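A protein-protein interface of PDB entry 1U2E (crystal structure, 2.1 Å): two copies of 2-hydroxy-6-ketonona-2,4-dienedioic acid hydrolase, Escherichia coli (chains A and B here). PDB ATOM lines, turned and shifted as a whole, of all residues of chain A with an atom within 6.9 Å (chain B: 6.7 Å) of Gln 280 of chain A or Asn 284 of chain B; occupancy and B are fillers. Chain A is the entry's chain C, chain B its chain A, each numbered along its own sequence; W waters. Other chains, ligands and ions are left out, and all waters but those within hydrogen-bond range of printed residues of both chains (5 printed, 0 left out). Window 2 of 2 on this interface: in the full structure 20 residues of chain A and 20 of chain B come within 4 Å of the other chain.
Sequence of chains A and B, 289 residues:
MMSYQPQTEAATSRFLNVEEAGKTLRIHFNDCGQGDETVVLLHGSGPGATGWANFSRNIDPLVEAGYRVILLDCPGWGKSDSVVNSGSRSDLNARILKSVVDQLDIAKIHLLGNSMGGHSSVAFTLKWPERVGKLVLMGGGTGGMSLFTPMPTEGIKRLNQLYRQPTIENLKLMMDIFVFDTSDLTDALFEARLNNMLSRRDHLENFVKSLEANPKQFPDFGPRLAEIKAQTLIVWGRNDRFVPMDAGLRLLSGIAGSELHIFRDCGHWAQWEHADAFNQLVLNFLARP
OD1 of Asn 284 of chain B sits close to NE2 of Gln 280 of chain A (3.1 Å). OD1 of Asn 284 of chain B lies within hydrogen-bond range of ND2 of Asn 284 of chain A (2.7 Å).
The side-chain amino group (NZ) of Lys 134 of chain B is in hydrogen-bond range of the backbone carbonyl oxygen (O) of Arg 288 of chain B (2.9 Å). The side-chain amide nitrogen of Asn 284 of chain B lies close to the backbone carbonyl oxygen of Gln 280 of chain B, 3.4 Å away. OD1 of Asn 284 of chain A sits close to O of Gln 280 of chain A.
Ala 277 of chain A touches Arg 288 of chain B (CB to NH2, 3.7 Å). Leu 281 of chain B touches Leu 281 of chain A (CD2 to CD2, 3.96 Å). CD of Gln 280 of chain B touches ND2 of Asn 284 of chain A, at 3.4 Å.
Of chain B, only Asn 284 (3.1 Å) comes within 4 Å of Gln 280 of chain A. Of chain A, only Gln 280 and Asn 284 come within 4 Å of Asn 284 of chain B. Printed residues of chain A within 4 Å of Leu 281 of chain B: Leu 281 (3.96 Å). Of the printed residues of chain B, Ala 277 of chain A touches Arg 288 (3.7 Å). Of the printed residues of chain B, Asn 284 of chain A touches Gln 280 and Asn 284. Of the printed residues of chain A, Arg 288 of chain B touches Ala 277 (3.7 Å). The nearest residue of chain B that does not touch Gln 280 of chain A is Arg 288 of chain B (4.9 Å). The nearest residue of chain A that does not touch Asn 284 of chain B is Leu 281 of chain A (5.8 Å). The nearest printed residue of chain A that does not touch Leu 281 of chain B is Asn 284 of chain A (5.7 Å).
Hydrophobic or aromatic side chains of chain A within 4 Å of the printed part of chain B: Ala 277 and Leu 281. Of the 12 printed residues of chain B, 4 touch a printed residue of chain A. Along chain B the printed residues that touch a printed residue of chain A span positions 280 to 288. Among the printed residues, 5 pairs touch across the chains.
Gln 280 of chain A touches Asn 284 of chain B, and with the chains exchanged Asn 284 of chain A touches Gln 280 of chain B. Leu 281 of chain A touches its own counterpart, Leu 281 of chain B. Asn 284 of chain A touches its own counterpart, Asn 284 of chain B. Of the 5 pairs that touch across the chains among the printed residues, 4 have their exchanged pair printed and touching as well.
Water W1 lies within hydrogen-bond range of the backbone carbonyl oxygen (O) of Asn 284 of chain B (2.5 Å) and the side-chain amide nitrogen (NE2) of Gln 280 of chain A (3.1 Å). Water W5 lies within hydrogen-bond range of O of Asn 284 of chain A (2.6 Å) and NE2 of Gln 280 of chain B (2.7 Å). Water W3 lies within hydrogen-bond range of the side-chain amide oxygen (OE1) of Gln 280 of chain B (2.6 Å) and the backbone carbonyl oxygen (O) of Asn 284 of chain A (3.5 Å). Water W2 lies within hydrogen-bond range of NE of Arg 288 of chain B (2.7 Å), OE1 of Gln 280 of chain A (2.9 Å), N of Phe 285 of chain B (3.3 Å) and O of Asn 284 of chain B (3.5 Å). Water W4 lies within hydrogen-bond range of the side-chain amide oxygen of Asn 284 of chain A (3.0 Å) and the side-chain amide nitrogen of Asn 284 of chain B (3.2 Å).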
ATOM      1  N   PRO A  61      32.016  18.207  12.124  1.00  0.00           N
ATOM      2  CA  PRO A  61      31.728  16.806  12.446  1.00  0.00           C
ATOM      3  C   PRO A  61      32.922  15.925  12.078  1.00  0.00           C
ATOM      4  O   PRO A  61      33.181  14.901  12.709  1.00  0.00           O
ATOM      5  CB  PRO A  61      30.492  16.508  11.601  1.00  0.00           C
ATOM      6  CG  PRO A  61      29.800  17.847  11.533  1.00  0.00           C
ATOM      7  CD  PRO A  61      30.957  18.787  11.277  1.00  0.00           C
ATOM      8  N   HIS A 274      21.066  18.853   3.207  1.00  0.00           N
ATOM      9  CA  HIS A 274      20.788  17.750   4.125  1.00  0.00           C
ATOM     10  C   HIS A 274      22.062  17.443   4.899  1.00  0.00           C
ATOM     11  O   HIS A 274      22.501  16.293   4.977  1.00  0.00           O
ATOM     12  CB  HIS A 274      20.329  16.517   3.337  1.00  0.00           C
ATOM     13  CG  HIS A 274      19.023  16.710   2.633  1.00  0.00           C
ATOM     14  ND1 HIS A 274      17.814  16.385   3.208  1.00  0.00           N
ATOM     15  CD2 HIS A 274      18.732  17.249   1.424  1.00  0.00           C
ATOM     16  CE1 HIS A 274      16.834  16.720   2.387  1.00  0.00           C
ATOM     17  NE2 HIS A 274      17.364  17.246   1.297  1.00  0.00           N
ATOM     18  N   ALA A 275      22.642  18.495   5.469  1.00  0.00           N
ATOM     19  CA  ALA A 275      23.884  18.412   6.226  1.00  0.00           C
ATOM     20  C   ALA A 275      23.960  17.267   7.228  1.00  0.00           C
ATOM     21  O   ALA A 275      24.880  16.449   7.172  1.00  0.00           O
ATOM     22  CB  ALA A 275      24.142  19.739   6.930  1.00  0.00           C
ATOM     23  N   ASP A 276      23.002  17.195   8.143  1.00  0.00           N
ATOM     24  CA  ASP A 276      23.025  16.132   9.140  1.00  0.00           C
ATOM     25  C   ASP A 276      22.972  14.736   8.535  1.00  0.00           C
ATOM     26  O   ASP A 276      23.746  13.859   8.922  1.00  0.00           O
ATOM     27  CB  ASP A 276      21.892  16.312  10.147  1.00  0.00           C
ATOM     28  CG  ASP A 276      22.076  17.550  10.998  1.00  0.00           C
ATOM     29  OD1 ASP A 276      23.231  17.837  11.369  1.00  0.00           O
ATOM     30  OD2 ASP A 276      21.078  18.231  11.303  1.00  0.00           O
ATOM     31  N   ALA A 277      22.062  14.514   7.594  1.00  0.00           N
ATOM     32  CA  ALA A 277      21.985  13.198   6.975  1.00  0.00           C
ATOM     33  C   ALA A 277      23.316  12.935   6.273  1.00  0.00           C
ATOM     34  O   ALA A 277      23.857  11.830   6.340  1.00  0.00           O
ATOM     35  CB  ALA A 277      20.832  13.141   5.973  1.00  0.00           C
ATOM     36  N   PHE A 278      23.848  13.966   5.620  1.00  0.00           N
ATOM     37  CA  PHE A 278      25.112  13.848   4.892  1.00  0.00           C
ATOM     38  C   PHE A 278      26.298  13.559   5.803  1.00  0.00           C
ATOM     39  O   PHE A 278      27.032  12.600   5.585  1.00  0.00           O
ATOM     40  CB  PHE A 278      25.403  15.122   4.101  1.00  0.00           C
ATOM     41  CG  PHE A 278      26.703  15.077   3.347  1.00  0.00           C
ATOM     42  CD1 PHE A 278      26.804  14.372   2.151  1.00  0.00           C
ATOM     43  CD2 PHE A 278      27.840  15.712   3.853  1.00  0.00           C
ATOM     44  CE1 PHE A 278      28.024  14.294   1.467  1.00  0.00           C
ATOM     45  CE2 PHE A 278      29.060  15.644   3.181  1.00  0.00           C
ATOM     46  CZ  PHE A 278      29.154  14.930   1.982  1.00  0.00           C
ATOM     47  N   ASN A 279      26.493  14.387   6.825  1.00  0.00           N
ATOM     48  CA  ASN A 279      27.616  14.178   7.725  1.00  0.00           C
ATOM     49  C   ASN A 279      27.546  12.800   8.373  1.00  0.00           C
ATOM     50  O   ASN A 279      28.570  12.176   8.644  1.00  0.00           O
ATOM     51  CB  ASN A 279      27.660  15.273   8.796  1.00  0.00           C
ATOM     52  CG  ASN A 279      27.918  16.654   8.206  1.00  0.00           C
ATOM     53  OD1 ASN A 279      28.656  16.797   7.228  1.00  0.00           O
ATOM     54  ND2 ASN A 279      27.323  17.679   8.809  1.00  0.00           N
ATOM     55  N   GLN A 280      26.332  12.314   8.605  1.00  0.00           N
ATOM     56  CA  GLN A 280      26.169  11.009   9.217  1.00  0.00           C
ATOM     57  C   GLN A 280      26.531   9.898   8.224  1.00  0.00           C
ATOM     58  O   GLN A 280      27.123   8.884   8.603  1.00  0.00           O
ATOM     59  CB  GLN A 280      24.729  10.840   9.712  1.00  0.00           C
ATOM     60  CG  GLN A 280      24.433   9.459  10.265  1.00  0.00           C
ATOM     61  CD  GLN A 280      22.984   9.297  10.666  1.00  0.00           C
ATOM     62  OE1 GLN A 280      22.078   9.486   9.853  1.00  0.00           O
ATOM     63  NE2 GLN A 280      22.756   8.945  11.930  1.00  0.00           N
ATOM     64  N   LEU A 281      26.173  10.081   6.954  1.00  0.00           N
ATOM     65  CA  LEU A 281      26.497   9.079   5.940  1.00  0.00           C
ATOM     66  C   LEU A 281      28.010   9.020   5.773  1.00  0.00           C
ATOM     67  O   LEU A 281      28.596   7.938   5.724  1.00  0.00           O
ATOM     68  CB  LEU A 281      25.852   9.429   4.592  1.00  0.00           C
ATOM     69  CG  LEU A 281      24.394   9.050   4.361  1.00  0.00           C
ATOM     70  CD1 LEU A 281      23.868   9.777   3.128  1.00  0.00           C
ATOM     71  CD2 LEU A 281      24.279   7.534   4.196  1.00  0.00           C
ATOM     72  N   VAL A 282      28.631  10.193   5.684  1.00  0.00           N
ATOM     73  CA  VAL A 282      30.077  10.288   5.518  1.00  0.00           C
ATOM     74  C   VAL A 282      30.850   9.687   6.687  1.00  0.00           C
ATOM     75  O   VAL A 282      31.731   8.867   6.477  1.00  0.00           O
ATOM     76  CB  VAL A 282      30.526  11.749   5.304  1.00  0.00           C
ATOM     77  CG1 VAL A 282      32.049  11.842   5.393  1.00  0.00           C
ATOM     78  CG2 VAL A 282      30.071  12.230   3.929  1.00  0.00           C
ATOM     79  N   LEU A 283      30.526  10.088   7.915  1.00  0.00           N
ATOM     80  CA  LEU A 283      31.202   9.534   9.082  1.00  0.00           C
ATOM     81  C   LEU A 283      31.054   8.003   9.118  1.00  0.00           C
ATOM     82  O   LEU A 283      32.025   7.278   9.363  1.00  0.00           O
ATOM     83  CB  LEU A 283      30.642  10.157  10.361  1.00  0.00           C
ATOM     84  CG  LEU A 283      31.224  11.509  10.806  1.00  0.00           C
ATOM     85  CD1 LEU A 283      31.256  12.482   9.646  1.00  0.00           C
ATOM     86  CD2 LEU A 283      30.373  12.082  11.941  1.00  0.00           C
ATOM     87  N   ASN A 284      29.846   7.511   8.867  1.00  0.00           N
ATOM     88  CA  ASN A 284      29.614   6.074   8.838  1.00  0.00           C
ATOM     89  C   ASN A 284      30.504   5.444   7.768  1.00  0.00           C
ATOM     90  O   ASN A 284      31.169   4.437   8.012  1.00  0.00           O
ATOM     91  CB  ASN A 284      28.162   5.755   8.482  1.00  0.00           C
ATOM     92  CG  ASN A 284      27.205   6.003   9.620  1.00  0.00           C
ATOM     93  OD1 ASN A 284      27.603   6.397  10.714  1.00  0.00           O
ATOM     94  ND2 ASN A 284      25.926   5.763   9.365  1.00  0.00           N
ATOM     95  N   PHE A 285      30.498   6.040   6.579  1.00  0.00           N
ATOM     96  CA  PHE A 285      31.282   5.526   5.462  1.00  0.00           C
ATOM     97  C   PHE A 285      32.771   5.535   5.779  1.00  0.00           C
ATOM     98  O   PHE A 285      33.446   4.516   5.665  1.00  0.00           O
ATOM     99  CB  PHE A 285      31.019   6.360   4.200  1.00  0.00           C
ATOM    100  CG  PHE A 285      31.406   5.666   2.922  1.00  0.00           C
ATOM    101  CD1 PHE A 285      30.716   4.536   2.499  1.00  0.00           C
ATOM    102  CD2 PHE A 285      32.479   6.124   2.158  1.00  0.00           C
ATOM    103  CE1 PHE A 285      31.094   3.860   1.327  1.00  0.00           C
ATOM    104  CE2 PHE A 285      32.864   5.462   0.990  1.00  0.00           C
ATOM    105  CZ  PHE A 285      32.170   4.326   0.574  1.00  0.00           C
ATOM    106  N   LYS B 134       7.773   5.614  10.559  1.00  0.00           N
ATOM    107  CA  LYS B 134       8.664   5.715   9.416  1.00  0.00           C
ATOM    108  C   LYS B 134       8.455   4.567   8.453  1.00  0.00           C
ATOM    109  O   LYS B 134       8.057   3.472   8.857  1.00  0.00           O
ATOM    110  CB  LYS B 134      10.112   5.769   9.885  1.00  0.00           C
ATOM    111  CG  LYS B 134      10.470   7.109  10.516  1.00  0.00           C
ATOM    112  CD  LYS B 134      11.856   7.095  11.124  1.00  0.00           C
ATOM    113  CE  LYS B 134      12.264   8.490  11.588  1.00  0.00           C
ATOM    114  NZ  LYS B 134      11.341   9.056  12.597  1.00  0.00           N
ATOM    115  N   PHE B 278      23.007  -1.972   5.734  1.00  0.00           N
ATOM    116  CA  PHE B 278      21.558  -1.795   5.724  1.00  0.00           C
ATOM    117  C   PHE B 278      21.062  -1.515   7.143  1.00  0.00           C
ATOM    118  O   PHE B 278      20.340  -0.545   7.373  1.00  0.00           O
ATOM    119  CB  PHE B 278      20.872  -3.054   5.180  1.00  0.00           C
ATOM    120  CG  PHE B 278      19.365  -3.017   5.266  1.00  0.00           C
ATOM    121  CD1 PHE B 278      18.614  -2.351   4.306  1.00  0.00           C
ATOM    122  CD2 PHE B 278      18.699  -3.667   6.303  1.00  0.00           C
ATOM    123  CE1 PHE B 278      17.221  -2.337   4.374  1.00  0.00           C
ATOM    124  CE2 PHE B 278      17.309  -3.658   6.382  1.00  0.00           C
ATOM    125  CZ  PHE B 278      16.567  -2.991   5.410  1.00  0.00           C
ATOM    126  N   ASN B 279      21.455  -2.365   8.092  1.00  0.00           N
ATOM    127  CA  ASN B 279      21.030  -2.191   9.473  1.00  0.00           C
ATOM    128  C   ASN B 279      21.438  -0.820   9.975  1.00  0.00           C
ATOM    129  O   ASN B 279      20.674  -0.154  10.681  1.00  0.00           O
ATOM    130  CB  ASN B 279      21.628  -3.274  10.371  1.00  0.00           C
ATOM    131  CG  ASN B 279      21.033  -4.629  10.112  1.00  0.00           C
ATOM    132  OD1 ASN B 279      19.887  -4.738   9.681  1.00  0.00           O
ATOM    133  ND2 ASN B 279      21.799  -5.679  10.385  1.00  0.00           N
ATOM    134  N   GLN B 280      22.641  -0.398   9.603  1.00  0.00           N
ATOM    135  CA  GLN B 280      23.150   0.909  10.005  1.00  0.00           C
ATOM    136  C   GLN B 280      22.267   2.014   9.422  1.00  0.00           C
ATOM    137  O   GLN B 280      21.893   2.948  10.127  1.00  0.00           O
ATOM    138  CB  GLN B 280      24.589   1.072   9.520  1.00  0.00           C
ATOM    139  CG  GLN B 280      25.247   2.393   9.880  1.00  0.00           C
ATOM    140  CD  GLN B 280      26.686   2.442   9.400  1.00  0.00           C
ATOM    141  OE1 GLN B 280      26.958   2.263   8.213  1.00  0.00           O
ATOM    142  NE2 GLN B 280      27.612   2.672  10.319  1.00  0.00           N
ATOM    143  N   LEU B 281      21.942   1.903   8.134  1.00  0.00           N
ATOM    144  CA  LEU B 281      21.081   2.884   7.471  1.00  0.00           C
ATOM    145  C   LEU B 281      19.725   2.980   8.172  1.00  0.00           C
ATOM    146  O   LEU B 281      19.259   4.074   8.490  1.00  0.00           O
ATOM    147  CB  LEU B 281      20.845   2.503   5.999  1.00  0.00           C
ATOM    148  CG  LEU B 281      21.757   3.005   4.872  1.00  0.00           C
ATOM    149  CD1 LEU B 281      21.254   2.424   3.557  1.00  0.00           C
ATOM    150  CD2 LEU B 281      21.757   4.538   4.799  1.00  0.00           C
ATOM    151  N   VAL B 282      19.102   1.827   8.408  1.00  0.00           N
ATOM    152  CA  VAL B 282      17.790   1.764   9.056  1.00  0.00           C
ATOM    153  C   VAL B 282      17.801   2.313  10.476  1.00  0.00           C
ATOM    154  O   VAL B 282      16.955   3.134  10.832  1.00  0.00           O
ATOM    155  CB  VAL B 282      17.245   0.314   9.086  1.00  0.00           C
ATOM    156  CG1 VAL B 282      15.944   0.255   9.879  1.00  0.00           C
ATOM    157  CG2 VAL B 282      17.002  -0.168   7.675  1.00  0.00           C
ATOM    158  N   LEU B 283      18.759   1.864  11.282  1.00  0.00           N
ATOM    159  CA  LEU B 283      18.862   2.336  12.654  1.00  0.00           C
ATOM    160  C   LEU B 283      18.996   3.852  12.679  1.00  0.00           C
ATOM    161  O   LEU B 283      18.306   4.529  13.445  1.00  0.00           O
ATOM    162  CB  LEU B 283      20.050   1.669  13.352  1.00  0.00           C
ATOM    163  CG  LEU B 283      19.718   0.505  14.302  1.00  0.00           C
ATOM    164  CD1 LEU B 283      18.380  -0.134  13.948  1.00  0.00           C
ATOM    165  CD2 LEU B 283      20.851  -0.523  14.252  1.00  0.00           C
ATOM    166  N   ASN B 284      19.877   4.392  11.840  1.00  0.00           N
ATOM    167  CA  ASN B 284      20.044   5.842  11.776  1.00  0.00           C
ATOM    168  C   ASN B 284      18.707   6.472  11.391  1.00  0.00           C
ATOM    169  O   ASN B 284      18.242   7.425  12.021  1.00  0.00           O
ATOM    170  CB  ASN B 284      21.079   6.234  10.715  1.00  0.00           C
ATOM    171  CG  ASN B 284      22.502   5.978  11.152  1.00  0.00           C
ATOM    172  OD1 ASN B 284      23.446   6.271  10.417  1.00  0.00           O
ATOM    173  ND2 ASN B 284      22.671   5.430  12.351  1.00  0.00           N
ATOM    174  N   PHE B 285      18.092   5.919  10.351  1.00  0.00           N
ATOM    175  CA  PHE B 285      16.830   6.437   9.860  1.00  0.00           C
ATOM    176  C   PHE B 285      15.774   6.411  10.941  1.00  0.00           C
ATOM    177  O   PHE B 285      15.168   7.431  11.252  1.00  0.00           O
ATOM    178  CB  PHE B 285      16.349   5.635   8.655  1.00  0.00           C
ATOM    179  CG  PHE B 285      15.280   6.330   7.862  1.00  0.00           C
ATOM    180  CD1 PHE B 285      15.575   7.481   7.138  1.00  0.00           C
ATOM    181  CD2 PHE B 285      13.983   5.830   7.830  1.00  0.00           C
ATOM    182  CE1 PHE B 285      14.595   8.120   6.392  1.00  0.00           C
ATOM    183  CE2 PHE B 285      12.992   6.465   7.083  1.00  0.00           C
ATOM    184  CZ  PHE B 285      13.300   7.611   6.364  1.00  0.00           C
ATOM    185  N   LEU B 286      15.556   5.231  11.502  1.00  0.00           N
ATOM    186  CA  LEU B 286      14.581   5.046  12.565  1.00  0.00           C
ATOM    187  C   LEU B 286      14.816   5.975  13.749  1.00  0.00           C
ATOM    188  O   LEU B 286      13.886   6.292  14.478  1.00  0.00           O
ATOM    189  CB  LEU B 286      14.609   3.591  13.039  1.00  0.00           C
ATOM    190  CG  LEU B 286      13.479   2.671  12.564  1.00  0.00           C
ATOM    191  CD1 LEU B 286      13.006   3.043  11.159  1.00  0.00           C
ATOM    192  CD2 LEU B 286      13.967   1.236  12.630  1.00  0.00           C
ATOM    193  N   ALA B 287      16.054   6.425  13.931  1.00  0.00           N
ATOM    194  CA  ALA B 287      16.391   7.309  15.048  1.00  0.00           C
ATOM    195  C   ALA B 287      16.156   8.784  14.786  1.00  0.00           C
ATOM    196  O   ALA B 287      16.313   9.601  15.686  1.00  0.00           O
ATOM    197  CB  ALA B 287      17.845   7.099  15.465  1.00  0.00           C
ATOM    198  N   ARG B 288      15.794   9.144  13.562  1.00  0.00           N
ATOM    199  CA  ARG B 288      15.566  10.553  13.253  1.00  0.00           C
ATOM    200  C   ARG B 288      14.308  11.022  13.951  1.00  0.00           C
ATOM    201  O   ARG B 288      13.423  10.223  14.240  1.00  0.00           O
ATOM    202  CB  ARG B 288      15.379  10.769  11.750  1.00  0.00           C
ATOM    203  CG  ARG B 288      16.546  10.352  10.875  1.00  0.00           C
ATOM    204  CD  ARG B 288      16.232  10.656   9.407  1.00  0.00           C
ATOM    205  NE  ARG B 288      17.358  10.342   8.539  1.00  0.00           N
ATOM    206  CZ  ARG B 288      17.430  10.667   7.254  1.00  0.00           C
ATOM    207  NH1 ARG B 288      16.432  11.320   6.667  1.00  0.00           N
ATOM    208  NH2 ARG B 288      18.515  10.354   6.563  1.00  0.00           N
HETATM  209  O   HOH W   1      19.816   9.051  13.008  1.00  0.00           O
HETATM  210  O   HOH W   2      19.414   8.582   8.972  1.00  0.00           O
HETATM  211  O   HOH W   3      28.428   3.235   6.247  1.00  0.00           O
HETATM  212  O   HOH W   4      25.775   5.836  13.029  1.00  0.00           O
HETATM  213  O   HOH W   5      30.251   2.725   9.708  1.00  0.00           O
